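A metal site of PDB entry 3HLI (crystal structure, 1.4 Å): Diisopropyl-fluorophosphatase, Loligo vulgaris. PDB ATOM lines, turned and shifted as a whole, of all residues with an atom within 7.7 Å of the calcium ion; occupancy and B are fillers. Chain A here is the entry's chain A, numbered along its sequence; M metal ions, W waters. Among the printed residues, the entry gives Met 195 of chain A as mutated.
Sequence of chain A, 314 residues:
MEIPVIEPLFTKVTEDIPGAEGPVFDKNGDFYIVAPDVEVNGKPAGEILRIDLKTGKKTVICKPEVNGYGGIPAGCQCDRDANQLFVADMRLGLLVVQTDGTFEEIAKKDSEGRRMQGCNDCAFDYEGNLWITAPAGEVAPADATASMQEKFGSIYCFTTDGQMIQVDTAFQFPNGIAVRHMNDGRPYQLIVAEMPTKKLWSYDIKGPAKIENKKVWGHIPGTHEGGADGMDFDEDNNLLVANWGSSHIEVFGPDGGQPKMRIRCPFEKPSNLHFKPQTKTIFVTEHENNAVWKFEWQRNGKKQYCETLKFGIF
The side-chain amide nitrogen of Asn 272 is in hydrogen-bond range of the side-chain carboxylate of Glu 21, at 2.8 Å. The side-chain hydroxyl of Thr 133 lies within hydrogen-bond range of the backbone carbonyl oxygen of Asn 175, 2.7 Å away. The backbone carbonyl oxygen (O) of Asp 229 sits close to the backbone NH (N) of Gly 176 (2.9 Å). The backbone carbonyl oxygen (O) of Asn 120 sits at hydrogen-bond distance from the backbone NH (N) of Gly 75, 3.1 Å away. N of Asn 120 lies within hydrogen-bond range of O of Thr 133 (2.9 Å).
Water W1 lies within hydrogen-bond range of the side-chain carboxylate (OD2) of Asp 121 (2.7 Å) and the backbone NH (N) of Gly 230 (3.4 Å).
Four residues have an atom within 4 Å of the calcium ion: Glu 21, Asn 120, Asn 175 and Asp 229.
The calcium ion is bound by OE2 of Glu 21, OD1 of Asn 175, OD1 of Asp 229, water W1, water W2 and OD1 of Asn 120.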
ATOM      1  N   ALA A  20      11.853  15.017  -2.220  1.00  0.00           N
ATOM      2  CA  ALA A  20      12.956  14.974  -3.178  1.00  0.00           C
ATOM      3  C   ALA A  20      12.672  14.074  -4.372  1.00  0.00           C
ATOM      4  O   ALA A  20      12.477  12.865  -4.220  1.00  0.00           O
ATOM      5  CB  ALA A  20      14.235  14.510  -2.473  1.00  0.00           C
ATOM      6  N   GLU A  21      12.669  14.670  -5.558  1.00  0.00           N
ATOM      7  CA  GLU A  21      12.369  13.949  -6.785  1.00  0.00           C
ATOM      8  C   GLU A  21      12.982  14.615  -8.009  1.00  0.00           C
ATOM      9  O   GLU A  21      13.725  15.595  -7.888  1.00  0.00           O
ATOM     10  CB  GLU A  21      10.847  13.859  -6.972  1.00  0.00           C
ATOM     11  CG  GLU A  21      10.251  12.480  -6.723  1.00  0.00           C
ATOM     12  CD  GLU A  21      10.363  11.578  -7.935  1.00  0.00           C
ATOM     13  OE1 GLU A  21      11.136  11.903  -8.865  1.00  0.00           O
ATOM     14  OE2 GLU A  21       9.663  10.541  -7.958  1.00  0.00           O
ATOM     15  N   GLY A  22      12.656  14.073  -9.165  1.00  0.00           N
ATOM     16  CA  GLY A  22      13.098  14.607 -10.449  1.00  0.00           C
ATOM     17  C   GLY A  22      14.521  15.070 -10.633  1.00  0.00           C
ATOM     18  O   GLY A  22      14.742  16.184 -11.130  1.00  0.00           O
ATOM     19  N   ALA A  74       7.181  17.161  -9.997  1.00  0.00           N
ATOM     20  CA  ALA A  74       7.622  15.840  -9.563  1.00  0.00           C
ATOM     21  C   ALA A  74       8.654  15.103 -10.411  1.00  0.00           C
ATOM     22  O   ALA A  74       9.308  14.191  -9.915  1.00  0.00           O
ATOM     23  CB  ALA A  74       6.394  14.942  -9.372  1.00  0.00           C
ATOM     24  N   GLY A  75       8.769  15.457 -11.683  1.00  0.00           N
ATOM     25  CA  GLY A  75       9.722  14.763 -12.542  1.00  0.00           C
ATOM     26  C   GLY A  75      10.250  15.688 -13.621  1.00  0.00           C
ATOM     27  O   GLY A  75       9.544  16.616 -14.023  1.00  0.00           O
ATOM     28  N   MET A  90       2.254  17.303 -10.713  1.00  0.00           N
ATOM     29  CA  MET A  90       1.067  16.583 -10.258  1.00  0.00           C
ATOM     30  C   MET A  90      -0.210  17.422 -10.163  1.00  0.00           C
ATOM     31  O   MET A  90      -1.302  16.872 -10.069  1.00  0.00           O
ATOM     32  CB  MET A  90       1.350  15.909  -8.906  1.00  0.00           C
ATOM     33  CG  MET A  90       2.343  14.744  -8.998  1.00  0.00           C
ATOM     34  SD  MET A  90       1.641  13.237  -9.701  1.00  0.00           S
ATOM     35  CE  MET A  90       0.755  12.594  -8.263  1.00  0.00           C
ATOM     36  N   ASN A 120       3.525  12.864 -13.230  1.00  0.00           N
ATOM     37  CA  ASN A 120       4.560  12.494 -12.253  1.00  0.00           C
ATOM     38  C   ASN A 120       5.991  12.468 -12.795  1.00  0.00           C
ATOM     39  O   ASN A 120       6.890  13.068 -12.212  1.00  0.00           O
ATOM     40  CB  ASN A 120       4.199  11.132 -11.644  1.00  0.00           C
ATOM     41  CG  ASN A 120       5.110  10.751 -10.504  1.00  0.00           C
ATOM     42  OD1 ASN A 120       6.291  10.487 -10.706  1.00  0.00           O
ATOM     43  ND2 ASN A 120       4.572  10.737  -9.294  1.00  0.00           N
ATOM     44  N   ASP A 121       6.208  11.753 -13.896  1.00  0.00           N
ATOM     45  CA  ASP A 121       7.555  11.682 -14.470  1.00  0.00           C
ATOM     46  C   ASP A 121       7.448  11.658 -15.982  1.00  0.00           C
ATOM     47  O   ASP A 121       6.358  11.499 -16.541  1.00  0.00           O
ATOM     48  CB  ASP A 121       8.283  10.423 -13.965  1.00  0.00           C
ATOM     49  CG  ASP A 121       9.806  10.608 -13.888  1.00  0.00           C
ATOM     50  OD1 ASP A 121      10.332  11.629 -14.390  1.00  0.00           O
ATOM     51  OD2 ASP A 121      10.479   9.725 -13.309  1.00  0.00           O
ATOM     52  N   CYS A 122       8.576  11.813 -16.660  1.00  0.00           N
ATOM     53  CA  CYS A 122       8.584  11.797 -18.108  1.00  0.00           C
ATOM     54  C   CYS A 122       9.934  11.345 -18.644  1.00  0.00           C
ATOM     55  O   CYS A 122      10.945  11.386 -17.944  1.00  0.00           O
ATOM     56  CB  CYS A 122       8.209  13.184 -18.668  1.00  0.00           C
ATOM     57  SG  CYS A 122       9.213  14.582 -18.084  1.00  0.00           S
ATOM     58  N   THR A 133       3.947  10.034 -17.472  1.00  0.00           N
ATOM     59  CA  THR A 133       3.018   9.293 -16.625  1.00  0.00           C
ATOM     60  C   THR A 133       2.126  10.312 -15.915  1.00  0.00           C
ATOM     61  O   THR A 133       2.585  11.390 -15.517  1.00  0.00           O
ATOM     62  CB  THR A 133       3.743   8.429 -15.571  1.00  0.00           C
ATOM     63  OG1 THR A 133       4.582   9.254 -14.752  1.00  0.00           O
ATOM     64  CG2 THR A 133       4.574   7.355 -16.247  1.00  0.00           C
ATOM     65  N   PRO A 135      -0.506   9.880 -12.963  1.00  0.00           N
ATOM     66  CA  PRO A 135      -1.235   9.140 -11.925  1.00  0.00           C
ATOM     67  C   PRO A 135      -2.261   9.956 -11.149  1.00  0.00           C
ATOM     68  O   PRO A 135      -3.108   9.384 -10.456  1.00  0.00           O
ATOM     69  CB  PRO A 135      -0.106   8.644 -11.024  1.00  0.00           C
ATOM     70  CG  PRO A 135       0.838   9.816 -11.045  1.00  0.00           C
ATOM     71  CD  PRO A 135       0.859  10.217 -12.520  1.00  0.00           C
ATOM     72  N   PHE A 173      -1.660   4.096 -10.509  1.00  0.00           N
ATOM     73  CA  PHE A 173      -0.533   4.958 -10.186  1.00  0.00           C
ATOM     74  C   PHE A 173       0.741   4.742 -11.002  1.00  0.00           C
ATOM     75  O   PHE A 173       1.779   4.295 -10.499  1.00  0.00           O
ATOM     76  CB  PHE A 173      -0.204   4.892  -8.695  1.00  0.00           C
ATOM     77  CG  PHE A 173       0.329   6.188  -8.155  1.00  0.00           C
ATOM     78  CD1 PHE A 173       1.673   6.514  -8.293  1.00  0.00           C
ATOM     79  CD2 PHE A 173      -0.526   7.113  -7.568  1.00  0.00           C
ATOM     80  CE1 PHE A 173       2.158   7.747  -7.857  1.00  0.00           C
ATOM     81  CE2 PHE A 173      -0.059   8.347  -7.118  1.00  0.00           C
ATOM     82  CZ  PHE A 173       1.292   8.664  -7.269  1.00  0.00           C
ATOM     83  N   PRO A 174       0.673   5.055 -12.300  1.00  0.00           N
ATOM     84  CA  PRO A 174       1.843   4.920 -13.169  1.00  0.00           C
ATOM     85  C   PRO A 174       2.848   5.925 -12.609  1.00  0.00           C
ATOM     86  O   PRO A 174       2.456   7.033 -12.231  1.00  0.00           O
ATOM     87  CB  PRO A 174       1.307   5.308 -14.548  1.00  0.00           C
ATOM     88  CG  PRO A 174       0.170   6.252 -14.216  1.00  0.00           C
ATOM     89  CD  PRO A 174      -0.486   5.578 -13.048  1.00  0.00           C
ATOM     90  N   ASN A 175       4.117   5.547 -12.546  1.00  0.00           N
ATOM     91  CA  ASN A 175       5.095   6.449 -11.956  1.00  0.00           C
ATOM     92  C   ASN A 175       6.330   6.633 -12.843  1.00  0.00           C
ATOM     93  O   ASN A 175       6.375   7.554 -13.654  1.00  0.00           O
ATOM     94  CB  ASN A 175       5.471   5.911 -10.570  1.00  0.00           C
ATOM     95  CG  ASN A 175       6.008   6.991  -9.662  1.00  0.00           C
ATOM     96  OD1 ASN A 175       6.822   7.811 -10.089  1.00  0.00           O
ATOM     97  ND2 ASN A 175       5.563   7.010  -8.413  1.00  0.00           N
ATOM     98  N   GLY A 176       7.351   5.789 -12.669  1.00  0.00           N
ATOM     99  CA  GLY A 176       8.536   5.904 -13.506  1.00  0.00           C
ATOM    100  C   GLY A 176       8.235   5.513 -14.943  1.00  0.00           C
ATOM    101  O   GLY A 176       7.260   4.817 -15.218  1.00  0.00           O
ATOM    102  N   ILE A 177       9.087   5.967 -15.858  1.00  0.00           N
ATOM    103  CA  ILE A 177       8.904   5.680 -17.281  1.00  0.00           C
ATOM    104  C   ILE A 177      10.260   5.794 -17.974  1.00  0.00           C
ATOM    105  O   ILE A 177      11.098   6.606 -17.576  1.00  0.00           O
ATOM    106  CB  ILE A 177       7.848   6.659 -17.881  1.00  0.00           C
ATOM    107  CG1 ILE A 177       7.486   6.267 -19.318  1.00  0.00           C
ATOM    108  CG2 ILE A 177       8.357   8.084 -17.811  1.00  0.00           C
ATOM    109  CD1 ILE A 177       6.162   6.864 -19.801  1.00  0.00           C
ATOM    110  N   MET A 195       3.370   1.550  -9.871  1.00  0.00           N
ATOM    111  CA  MET A 195       3.890   1.412  -8.516  1.00  0.00           C
ATOM    112  C   MET A 195       3.334   0.389  -7.527  1.00  0.00           C
ATOM    113  O   MET A 195       4.015  -0.595  -7.221  1.00  0.00           O
ATOM    114  CB  MET A 195       3.935   2.781  -7.840  1.00  0.00           C
ATOM    115  CG  MET A 195       4.561   2.737  -6.470  1.00  0.00           C
ATOM    116  SD  MET A 195       4.834   4.367  -5.776  1.00  0.00           S
ATOM    117  CE  MET A 195       6.605   4.553  -6.009  1.00  0.00           C
ATOM    118  N   ALA A 228       7.920   0.357  -7.699  1.00  0.00           N
ATOM    119  CA  ALA A 228       8.733   1.087  -8.662  1.00  0.00           C
ATOM    120  C   ALA A 228       8.385   2.571  -8.771  1.00  0.00           C
ATOM    121  O   ALA A 228       7.233   2.933  -9.011  1.00  0.00           O
ATOM    122  CB  ALA A 228       8.639   0.436 -10.038  1.00  0.00           C
ATOM    123  N   ASP A 229       9.399   3.415  -8.595  1.00  0.00           N
ATOM    124  CA  ASP A 229       9.219   4.856  -8.710  1.00  0.00           C
ATOM    125  C   ASP A 229       9.996   5.250  -9.979  1.00  0.00           C
ATOM    126  O   ASP A 229       9.623   4.819 -11.071  1.00  0.00           O
ATOM    127  CB  ASP A 229       9.757   5.571  -7.463  1.00  0.00           C
ATOM    128  CG  ASP A 229       9.147   6.945  -7.266  1.00  0.00           C
ATOM    129  OD1 ASP A 229       8.847   7.612  -8.278  1.00  0.00           O
ATOM    130  OD2 ASP A 229       8.980   7.372  -6.101  1.00  0.00           O
ATOM    131  N   GLY A 230      11.067   6.030  -9.842  1.00  0.00           N
ATOM    132  CA  GLY A 230      11.834   6.444 -11.015  1.00  0.00           C
ATOM    133  C   GLY A 230      12.763   5.399 -11.621  1.00  0.00           C
ATOM    134  O   GLY A 230      13.169   4.452 -10.954  1.00  0.00           O
ATOM    135  N   MET A 231      13.106   5.590 -12.894  1.00  0.00           N
ATOM    136  CA  MET A 231      13.978   4.655 -13.599  1.00  0.00           C
ATOM    137  C   MET A 231      14.809   5.305 -14.688  1.00  0.00           C
ATOM    138  O   MET A 231      14.500   6.399 -15.157  1.00  0.00           O
ATOM    139  CB  MET A 231      13.130   3.558 -14.250  1.00  0.00           C
ATOM    140  CG  MET A 231      12.121   4.100 -15.247  1.00  0.00           C
ATOM    141  SD  MET A 231      11.170   2.800 -16.042  1.00  0.00           S
ATOM    142  CE  MET A 231      10.709   1.822 -14.582  1.00  0.00           C
ATOM    143  N   SER A 271      13.387   7.387  -4.451  1.00  0.00           N
ATOM    144  CA  SER A 271      12.285   7.842  -5.291  1.00  0.00           C
ATOM    145  C   SER A 271      12.664   7.970  -6.764  1.00  0.00           C
ATOM    146  O   SER A 271      11.846   7.678  -7.646  1.00  0.00           O
ATOM    147  CB  SER A 271      11.762   9.188  -4.785  1.00  0.00           C
ATOM    148  OG  SER A 271      12.777  10.177  -4.804  1.00  0.00           O
ATOM    149  N   ASN A 272      13.890   8.390  -7.043  1.00  0.00           N
ATOM    150  CA  ASN A 272      14.298   8.534  -8.426  1.00  0.00           C
ATOM    151  C   ASN A 272      15.819   8.567  -8.534  1.00  0.00           C
ATOM    152  O   ASN A 272      16.526   8.574  -7.520  1.00  0.00           O
ATOM    153  CB  ASN A 272      13.691   9.815  -9.012  1.00  0.00           C
ATOM    154  CG  ASN A 272      13.271   9.645 -10.458  1.00  0.00           C
ATOM    155  OD1 ASN A 272      13.921   8.920 -11.217  1.00  0.00           O
ATOM    156  ND2 ASN A 272      12.198  10.307 -10.844  1.00  0.00           N
ATOM    157  N   THR A 285      17.442  10.450  -5.336  1.00  0.00           N
ATOM    158  CA  THR A 285      16.583  11.221  -4.463  1.00  0.00           C
ATOM    159  C   THR A 285      15.835  10.190  -3.615  1.00  0.00           C
ATOM    160  O   THR A 285      15.575   9.081  -4.074  1.00  0.00           O
ATOM    161  CB  THR A 285      15.577  12.074  -5.263  1.00  0.00           C
ATOM    162  OG1 THR A 285      14.932  11.252  -6.250  1.00  0.00           O
ATOM    163  CG2 THR A 285      16.297  13.223  -5.956  1.00  0.00           C
ATOM    164  N   HIS A 287      12.880   9.635  -0.081  1.00  0.00           N
ATOM    165  CA  HIS A 287      11.888  10.187   0.826  1.00  0.00           C
ATOM    166  C   HIS A 287      11.983   9.821   2.295  1.00  0.00           C
ATOM    167  O   HIS A 287      11.163  10.259   3.095  1.00  0.00           O
ATOM    168  CB  HIS A 287      10.485   9.835   0.295  1.00  0.00           C
ATOM    169  CG  HIS A 287      10.200  10.408  -1.061  1.00  0.00           C
ATOM    170  ND1 HIS A 287       9.124  10.008  -1.831  1.00  0.00           N
ATOM    171  CD2 HIS A 287      10.824  11.379  -1.772  1.00  0.00           C
ATOM    172  CE1 HIS A 287       9.102  10.700  -2.959  1.00  0.00           C
ATOM    173  NE2 HIS A 287      10.125  11.542  -2.949  1.00  0.00           N
HETATM  174 CA    CA M   1       8.150   9.586  -9.385  1.00  0.00          CA
HETATM  175  O   HOH W   1       9.229   8.462 -11.249  1.00  0.00           O
HETATM  176  O   HOH W   2       8.823  11.562 -10.671  1.00  0.00           O
